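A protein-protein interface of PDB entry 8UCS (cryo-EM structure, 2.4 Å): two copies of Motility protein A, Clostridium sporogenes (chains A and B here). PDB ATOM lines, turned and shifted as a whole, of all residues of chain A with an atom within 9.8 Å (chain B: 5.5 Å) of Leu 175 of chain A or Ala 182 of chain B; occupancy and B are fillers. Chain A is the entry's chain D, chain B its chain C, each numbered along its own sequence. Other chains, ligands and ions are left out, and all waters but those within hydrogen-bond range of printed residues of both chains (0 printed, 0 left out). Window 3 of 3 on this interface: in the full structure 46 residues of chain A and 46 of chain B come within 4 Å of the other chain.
The backbone carbonyl oxygen of Thr 180 of chain B lies within hydrogen-bond range of the side-chain hydroxyl of Ser 183 of chain B (3.2 Å).
CG1 of Ile 169 of chain A touches O of Gly 186 of chain B, 3.8 Å away. Ala 182 of chain B touches Leu 172 of chain A (O to CD2, 3.3 Å). Leu 172 of chain A touches Ser 183 of chain B. Leu 172 of chain A touches Met 185 of chain B. Leu 172 of chain A touches Gly 186 of chain B (CD1 to N, 3.4 Å). Leu 175 of chain A touches Ala 182 of chain B.
Of the printed residues of chain B, Ile 169 of chain A touches Gly 186 (3.8 Å). Printed residues of chain B within 4 Å of Leu 172 of chain A: Ala 182 (3.3 Å), Ser 183 (3.7 Å), Met 185 (3.7 Å) and Gly 186 (3.4 Å). Ile 181 of chain B touches none of the printed residues of chain A. Ala 182 of chain B touches just these residues of chain A: Leu 172 (3.3 Å) and Leu 175 (3.6 Å). No residue of chain A comes within 4 Å of Gly 184 of chain B. Of the printed residues of chain A, Met 185 of chain B touches Leu 172. Of the printed residues of chain A, Gly 186 of chain B touches Ile 169 and Leu 172. The nearest residue of chain B that does not touch Leu 175 of chain A is Ser 183 of chain B (4.1 Å). The nearest residue of chain A that does not touch Ala 182 of chain B is Ala 173 of chain A (6.2 Å).
Hydrophobic or aromatic side chains of chain B within 4 Å of the printed part of chain A: Ala 182 and Met 185. Of the 16 printed residues of chain A, 3 touch a printed residue of chain B. Hydrophobic or aromatic side chains of chain A within 4 Å of the printed part of chain B: Ile 169, Leu 172 and Leu 175. Among the printed residues, no Asp or Glu carboxylate lies within 4 Å of a Lys or Arg side-chain nitrogen of the other chain.
6 positions are printed for both chains. Of the 6 pairs that touch across the chains among the printed residues, none has its exchanged pair printed and touching as well.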
ATOM      1  N   GLY A 167     -14.840   7.022  -0.789  1.00  0.00           N
ATOM      2  CA  GLY A 167     -15.493   5.740  -0.589  1.00  0.00           C
ATOM      3  C   GLY A 167     -16.229   5.638   0.733  1.00  0.00           C
ATOM      4  O   GLY A 167     -17.360   5.151   0.783  1.00  0.00           O
ATOM      5  N   LEU A 168     -15.598   6.087   1.822  1.00  0.00           N
ATOM      6  CA  LEU A 168     -16.244   6.025   3.130  1.00  0.00           C
ATOM      7  C   LEU A 168     -17.454   6.946   3.207  1.00  0.00           C
ATOM      8  O   LEU A 168     -18.484   6.573   3.777  1.00  0.00           O
ATOM      9  CB  LEU A 168     -15.243   6.353   4.235  1.00  0.00           C
ATOM     10  CG  LEU A 168     -15.690   5.980   5.653  1.00  0.00           C
ATOM     11  CD1 LEU A 168     -16.331   4.600   5.708  1.00  0.00           C
ATOM     12  CD2 LEU A 168     -14.519   6.060   6.619  1.00  0.00           C
ATOM     13  N   ILE A 169     -17.349   8.155   2.652  1.00  0.00           N
ATOM     14  CA  ILE A 169     -18.496   9.057   2.638  1.00  0.00           C
ATOM     15  C   ILE A 169     -19.631   8.448   1.827  1.00  0.00           C
ATOM     16  O   ILE A 169     -20.800   8.504   2.225  1.00  0.00           O
ATOM     17  CB  ILE A 169     -18.083  10.443   2.104  1.00  0.00           C
ATOM     18  CG1 ILE A 169     -17.280  11.200   3.163  1.00  0.00           C
ATOM     19  CG2 ILE A 169     -19.304  11.251   1.696  1.00  0.00           C
ATOM     20  CD1 ILE A 169     -16.475  12.356   2.612  1.00  0.00           C
ATOM     21  N   GLN A 170     -19.302   7.846   0.683  1.00  0.00           N
ATOM     22  CA  GLN A 170     -20.302   7.146  -0.116  1.00  0.00           C
ATOM     23  C   GLN A 170     -20.917   5.989   0.659  1.00  0.00           C
ATOM     24  O   GLN A 170     -22.138   5.798   0.651  1.00  0.00           O
ATOM     25  CB  GLN A 170     -19.665   6.630  -1.403  1.00  0.00           C
ATOM     26  CG  GLN A 170     -20.094   7.341  -2.655  1.00  0.00           C
ATOM     27  CD  GLN A 170     -19.557   6.663  -3.891  1.00  0.00           C
ATOM     28  OE1 GLN A 170     -18.776   7.246  -4.640  1.00  0.00           O
ATOM     29  NE2 GLN A 170     -19.965   5.417  -4.107  1.00  0.00           N
ATOM     30  N   MET A 171     -20.077   5.195   1.326  1.00  0.00           N
ATOM     31  CA  MET A 171     -20.566   4.020   2.039  1.00  0.00           C
ATOM     32  C   MET A 171     -21.483   4.407   3.191  1.00  0.00           C
ATOM     33  O   MET A 171     -22.529   3.783   3.399  1.00  0.00           O
ATOM     34  CB  MET A 171     -19.386   3.196   2.549  1.00  0.00           C
ATOM     35  CG  MET A 171     -19.559   1.702   2.394  1.00  0.00           C
ATOM     36  SD  MET A 171     -18.226   0.773   3.175  1.00  0.00           S
ATOM     37  CE  MET A 171     -18.211   1.517   4.803  1.00  0.00           C
ATOM     38  N   LEU A 172     -21.107   5.434   3.953  1.00  0.00           N
ATOM     39  CA  LEU A 172     -21.867   5.814   5.136  1.00  0.00           C
ATOM     40  C   LEU A 172     -23.131   6.594   4.806  1.00  0.00           C
ATOM     41  O   LEU A 172     -24.031   6.668   5.649  1.00  0.00           O
ATOM     42  CB  LEU A 172     -20.982   6.624   6.081  1.00  0.00           C
ATOM     43  CG  LEU A 172     -19.790   5.842   6.637  1.00  0.00           C
ATOM     44  CD1 LEU A 172     -18.859   6.739   7.436  1.00  0.00           C
ATOM     45  CD2 LEU A 172     -20.265   4.668   7.474  1.00  0.00           C
ATOM     46  N   ALA A 173     -23.226   7.172   3.611  1.00  0.00           N
ATOM     47  CA  ALA A 173     -24.406   7.924   3.216  1.00  0.00           C
ATOM     48  C   ALA A 173     -25.452   7.073   2.508  1.00  0.00           C
ATOM     49  O   ALA A 173     -26.559   7.562   2.258  1.00  0.00           O
ATOM     50  CB  ALA A 173     -24.010   9.096   2.313  1.00  0.00           C
ATOM     51  N   ASN A 174     -25.134   5.824   2.183  1.00  0.00           N
ATOM     52  CA  ASN A 174     -26.037   4.915   1.480  1.00  0.00           C
ATOM     53  C   ASN A 174     -26.032   3.547   2.148  1.00  0.00           C
ATOM     54  O   ASN A 174     -25.894   2.509   1.499  1.00  0.00           O
ATOM     55  CB  ASN A 174     -25.662   4.793   0.005  1.00  0.00           C
ATOM     56  CG  ASN A 174     -25.512   6.139  -0.675  1.00  0.00           C
ATOM     57  OD1 ASN A 174     -24.510   6.831  -0.501  1.00  0.00           O
ATOM     58  ND2 ASN A 174     -26.511   6.516  -1.462  1.00  0.00           N
ATOM     59  N   LEU A 175     -26.183   3.534   3.473  1.00  0.00           N
ATOM     60  CA  LEU A 175     -26.118   2.290   4.229  1.00  0.00           C
ATOM     61  C   LEU A 175     -27.295   1.360   3.962  1.00  0.00           C
ATOM     62  O   LEU A 175     -27.243   0.196   4.372  1.00  0.00           O
ATOM     63  CB  LEU A 175     -26.029   2.594   5.723  1.00  0.00           C
ATOM     64  CG  LEU A 175     -24.643   2.997   6.227  1.00  0.00           C
ATOM     65  CD1 LEU A 175     -24.761   3.815   7.496  1.00  0.00           C
ATOM     66  CD2 LEU A 175     -23.773   1.774   6.453  1.00  0.00           C
ATOM     67  N   THR A 176     -28.346   1.835   3.297  1.00  0.00           N
ATOM     68  CA  THR A 176     -29.469   0.984   2.930  1.00  0.00           C
ATOM     69  C   THR A 176     -29.332   0.377   1.541  1.00  0.00           C
ATOM     70  O   THR A 176     -30.161  -0.460   1.165  1.00  0.00           O
ATOM     71  CB  THR A 176     -30.782   1.773   3.007  1.00  0.00           C
ATOM     72  OG1 THR A 176     -30.758   2.838   2.049  1.00  0.00           O
ATOM     73  CG2 THR A 176     -30.974   2.354   4.400  1.00  0.00           C
ATOM     74  N   ASP A 177     -28.316   0.767   0.773  1.00  0.00           N
ATOM     75  CA  ASP A 177     -28.099   0.265  -0.580  1.00  0.00           C
ATOM     76  C   ASP A 177     -26.788  -0.512  -0.592  1.00  0.00           C
ATOM     77  O   ASP A 177     -25.711   0.077  -0.456  1.00  0.00           O
ATOM     78  CB  ASP A 177     -28.072   1.409  -1.593  1.00  0.00           C
ATOM     79  CG  ASP A 177     -27.979   0.921  -3.026  1.00  0.00           C
ATOM     80  OD1 ASP A 177     -28.162  -0.290  -3.261  1.00  0.00           O
ATOM     81  OD2 ASP A 177     -27.722   1.753  -3.921  1.00  0.00           O
ATOM     82  N   SER A 178     -26.882  -1.834  -0.761  1.00  0.00           N
ATOM     83  CA  SER A 178     -25.691  -2.675  -0.700  1.00  0.00           C
ATOM     84  C   SER A 178     -24.780  -2.463  -1.904  1.00  0.00           C
ATOM     85  O   SER A 178     -23.556  -2.572  -1.775  1.00  0.00           O
ATOM     86  CB  SER A 178     -26.092  -4.146  -0.591  1.00  0.00           C
ATOM     87  OG  SER A 178     -26.781  -4.576  -1.749  1.00  0.00           O
ATOM     88  N   SER A 179     -25.352  -2.172  -3.075  1.00  0.00           N
ATOM     89  CA  SER A 179     -24.531  -1.933  -4.258  1.00  0.00           C
ATOM     90  C   SER A 179     -23.693  -0.669  -4.106  1.00  0.00           C
ATOM     91  O   SER A 179     -22.519  -0.646  -4.495  1.00  0.00           O
ATOM     92  CB  SER A 179     -25.413  -1.848  -5.502  1.00  0.00           C
ATOM     93  OG  SER A 179     -25.969  -0.554  -5.645  1.00  0.00           O
ATOM     94  N   THR A 180     -24.278   0.395  -3.552  1.00  0.00           N
ATOM     95  CA  THR A 180     -23.510   1.610  -3.304  1.00  0.00           C
ATOM     96  C   THR A 180     -22.483   1.394  -2.198  1.00  0.00           C
ATOM     97  O   THR A 180     -21.386   1.962  -2.242  1.00  0.00           O
ATOM     98  CB  THR A 180     -24.445   2.767  -2.952  1.00  0.00           C
ATOM     99  OG1 THR A 180     -25.487   2.853  -3.931  1.00  0.00           O
ATOM    100  CG2 THR A 180     -23.681   4.078  -2.929  1.00  0.00           C
ATOM    101  N   ILE A 181     -22.824   0.580  -1.197  1.00  0.00           N
ATOM    102  CA  ILE A 181     -21.856   0.228  -0.162  1.00  0.00           C
ATOM    103  C   ILE A 181     -20.670  -0.501  -0.778  1.00  0.00           C
ATOM    104  O   ILE A 181     -19.508  -0.198  -0.482  1.00  0.00           O
ATOM    105  CB  ILE A 181     -22.527  -0.619   0.936  1.00  0.00           C
ATOM    106  CG1 ILE A 181     -23.398   0.257   1.837  1.00  0.00           C
ATOM    107  CG2 ILE A 181     -21.484  -1.364   1.753  1.00  0.00           C
ATOM    108  CD1 ILE A 181     -24.463  -0.515   2.577  1.00  0.00           C
ATOM    109  N   ALA A 182     -20.949  -1.471  -1.650  1.00  0.00           N
ATOM    110  CA  ALA A 182     -19.881  -2.230  -2.291  1.00  0.00           C
ATOM    111  C   ALA A 182     -19.032  -1.343  -3.192  1.00  0.00           C
ATOM    112  O   ALA A 182     -17.800  -1.453  -3.200  1.00  0.00           O
ATOM    113  CB  ALA A 182     -20.473  -3.390  -3.089  1.00  0.00           C
ATOM    114  N   ASP B 177     -29.053   5.578  17.713  1.00  0.00           N
ATOM    115  CA  ASP B 177     -28.905   4.173  17.357  1.00  0.00           C
ATOM    116  C   ASP B 177     -27.558   3.985  16.675  1.00  0.00           C
ATOM    117  O   ASP B 177     -26.881   4.951  16.314  1.00  0.00           O
ATOM    118  CB  ASP B 177     -30.050   3.694  16.458  1.00  0.00           C
ATOM    119  CG  ASP B 177     -30.344   4.655  15.325  1.00  0.00           C
ATOM    120  OD1 ASP B 177     -29.502   4.778  14.412  1.00  0.00           O
ATOM    121  OD2 ASP B 177     -31.419   5.291  15.349  1.00  0.00           O
ATOM    122  N   SER B 178     -27.174   2.718  16.507  1.00  0.00           N
ATOM    123  CA  SER B 178     -25.921   2.411  15.827  1.00  0.00           C
ATOM    124  C   SER B 178     -25.963   2.817  14.360  1.00  0.00           C
ATOM    125  O   SER B 178     -24.913   3.070  13.759  1.00  0.00           O
ATOM    126  CB  SER B 178     -25.605   0.922  15.958  1.00  0.00           C
ATOM    127  OG  SER B 178     -26.002   0.209  14.800  1.00  0.00           O
ATOM    128  N   SER B 179     -27.158   2.880  13.767  1.00  0.00           N
ATOM    129  CA  SER B 179     -27.262   3.263  12.363  1.00  0.00           C
ATOM    130  C   SER B 179     -27.029   4.758  12.176  1.00  0.00           C
ATOM    131  O   SER B 179     -26.327   5.169  11.245  1.00  0.00           O
ATOM    132  CB  SER B 179     -28.626   2.857  11.809  1.00  0.00           C
ATOM    133  OG  SER B 179     -28.537   2.533  10.433  1.00  0.00           O
ATOM    134  N   THR B 180     -27.610   5.588  13.047  1.00  0.00           N
ATOM    135  CA  THR B 180     -27.391   7.027  12.950  1.00  0.00           C
ATOM    136  C   THR B 180     -25.966   7.415  13.322  1.00  0.00           C
ATOM    137  O   THR B 180     -25.495   8.474  12.896  1.00  0.00           O
ATOM    138  CB  THR B 180     -28.394   7.783  13.829  1.00  0.00           C
ATOM    139  OG1 THR B 180     -28.602   9.097  13.299  1.00  0.00           O
ATOM    140  CG2 THR B 180     -27.893   7.900  15.259  1.00  0.00           C
ATOM    141  N   ILE B 181     -25.271   6.583  14.101  1.00  0.00           N
ATOM    142  CA  ILE B 181     -23.869   6.845  14.399  1.00  0.00           C
ATOM    143  C   ILE B 181     -23.017   6.636  13.155  1.00  0.00           C
ATOM    144  O   ILE B 181     -22.123   7.436  12.859  1.00  0.00           O
ATOM    145  CB  ILE B 181     -23.399   5.964  15.571  1.00  0.00           C
ATOM    146  CG1 ILE B 181     -23.853   6.557  16.905  1.00  0.00           C
ATOM    147  CG2 ILE B 181     -21.885   5.790  15.548  1.00  0.00           C
ATOM    148  CD1 ILE B 181     -23.357   5.795  18.112  1.00  0.00           C
ATOM    149  N   ALA B 182     -23.293   5.569  12.401  1.00  0.00           N
ATOM    150  CA  ALA B 182     -22.503   5.275  11.211  1.00  0.00           C
ATOM    151  C   ALA B 182     -22.606   6.392  10.182  1.00  0.00           C
ATOM    152  O   ALA B 182     -21.597   6.801   9.596  1.00  0.00           O
ATOM    153  CB  ALA B 182     -22.940   3.941  10.609  1.00  0.00           C
ATOM    154  N   SER B 183     -23.815   6.906   9.951  1.00  0.00           N
ATOM    155  CA  SER B 183     -23.971   8.033   9.043  1.00  0.00           C
ATOM    156  C   SER B 183     -23.436   9.329   9.638  1.00  0.00           C
ATOM    157  O   SER B 183     -23.199  10.287   8.894  1.00  0.00           O
ATOM    158  CB  SER B 183     -25.441   8.201   8.654  1.00  0.00           C
ATOM    159  OG  SER B 183     -26.239   8.516   9.780  1.00  0.00           O
ATOM    160  N   GLY B 184     -23.249   9.382  10.957  1.00  0.00           N
ATOM    161  CA  GLY B 184     -22.628  10.548  11.562  1.00  0.00           C
ATOM    162  C   GLY B 184     -21.166  10.692  11.190  1.00  0.00           C
ATOM    163  O   GLY B 184     -20.674  11.806  10.995  1.00  0.00           O
ATOM    164  N   MET B 185     -20.447   9.570  11.099  1.00  0.00           N
ATOM    165  CA  MET B 185     -19.050   9.619  10.678  1.00  0.00           C
ATOM    166  C   MET B 185     -18.917  10.141   9.254  1.00  0.00           C
ATOM    167  O   MET B 185     -17.944  10.831   8.927  1.00  0.00           O
ATOM    168  CB  MET B 185     -18.404   8.238  10.795  1.00  0.00           C
ATOM    169  CG  MET B 185     -17.860   7.903  12.174  1.00  0.00           C
ATOM    170  SD  MET B 185     -19.123   7.741  13.441  1.00  0.00           S
ATOM    171  CE  MET B 185     -18.138   7.898  14.926  1.00  0.00           C
ATOM    172  N   GLY B 186     -19.876   9.811   8.388  1.00  0.00           N
ATOM    173  CA  GLY B 186     -19.813  10.290   7.019  1.00  0.00           C
ATOM    174  C   GLY B 186     -19.883  11.801   6.933  1.00  0.00           C
ATOM    175  O   GLY B 186     -19.099  12.433   6.221  1.00  0.00           O
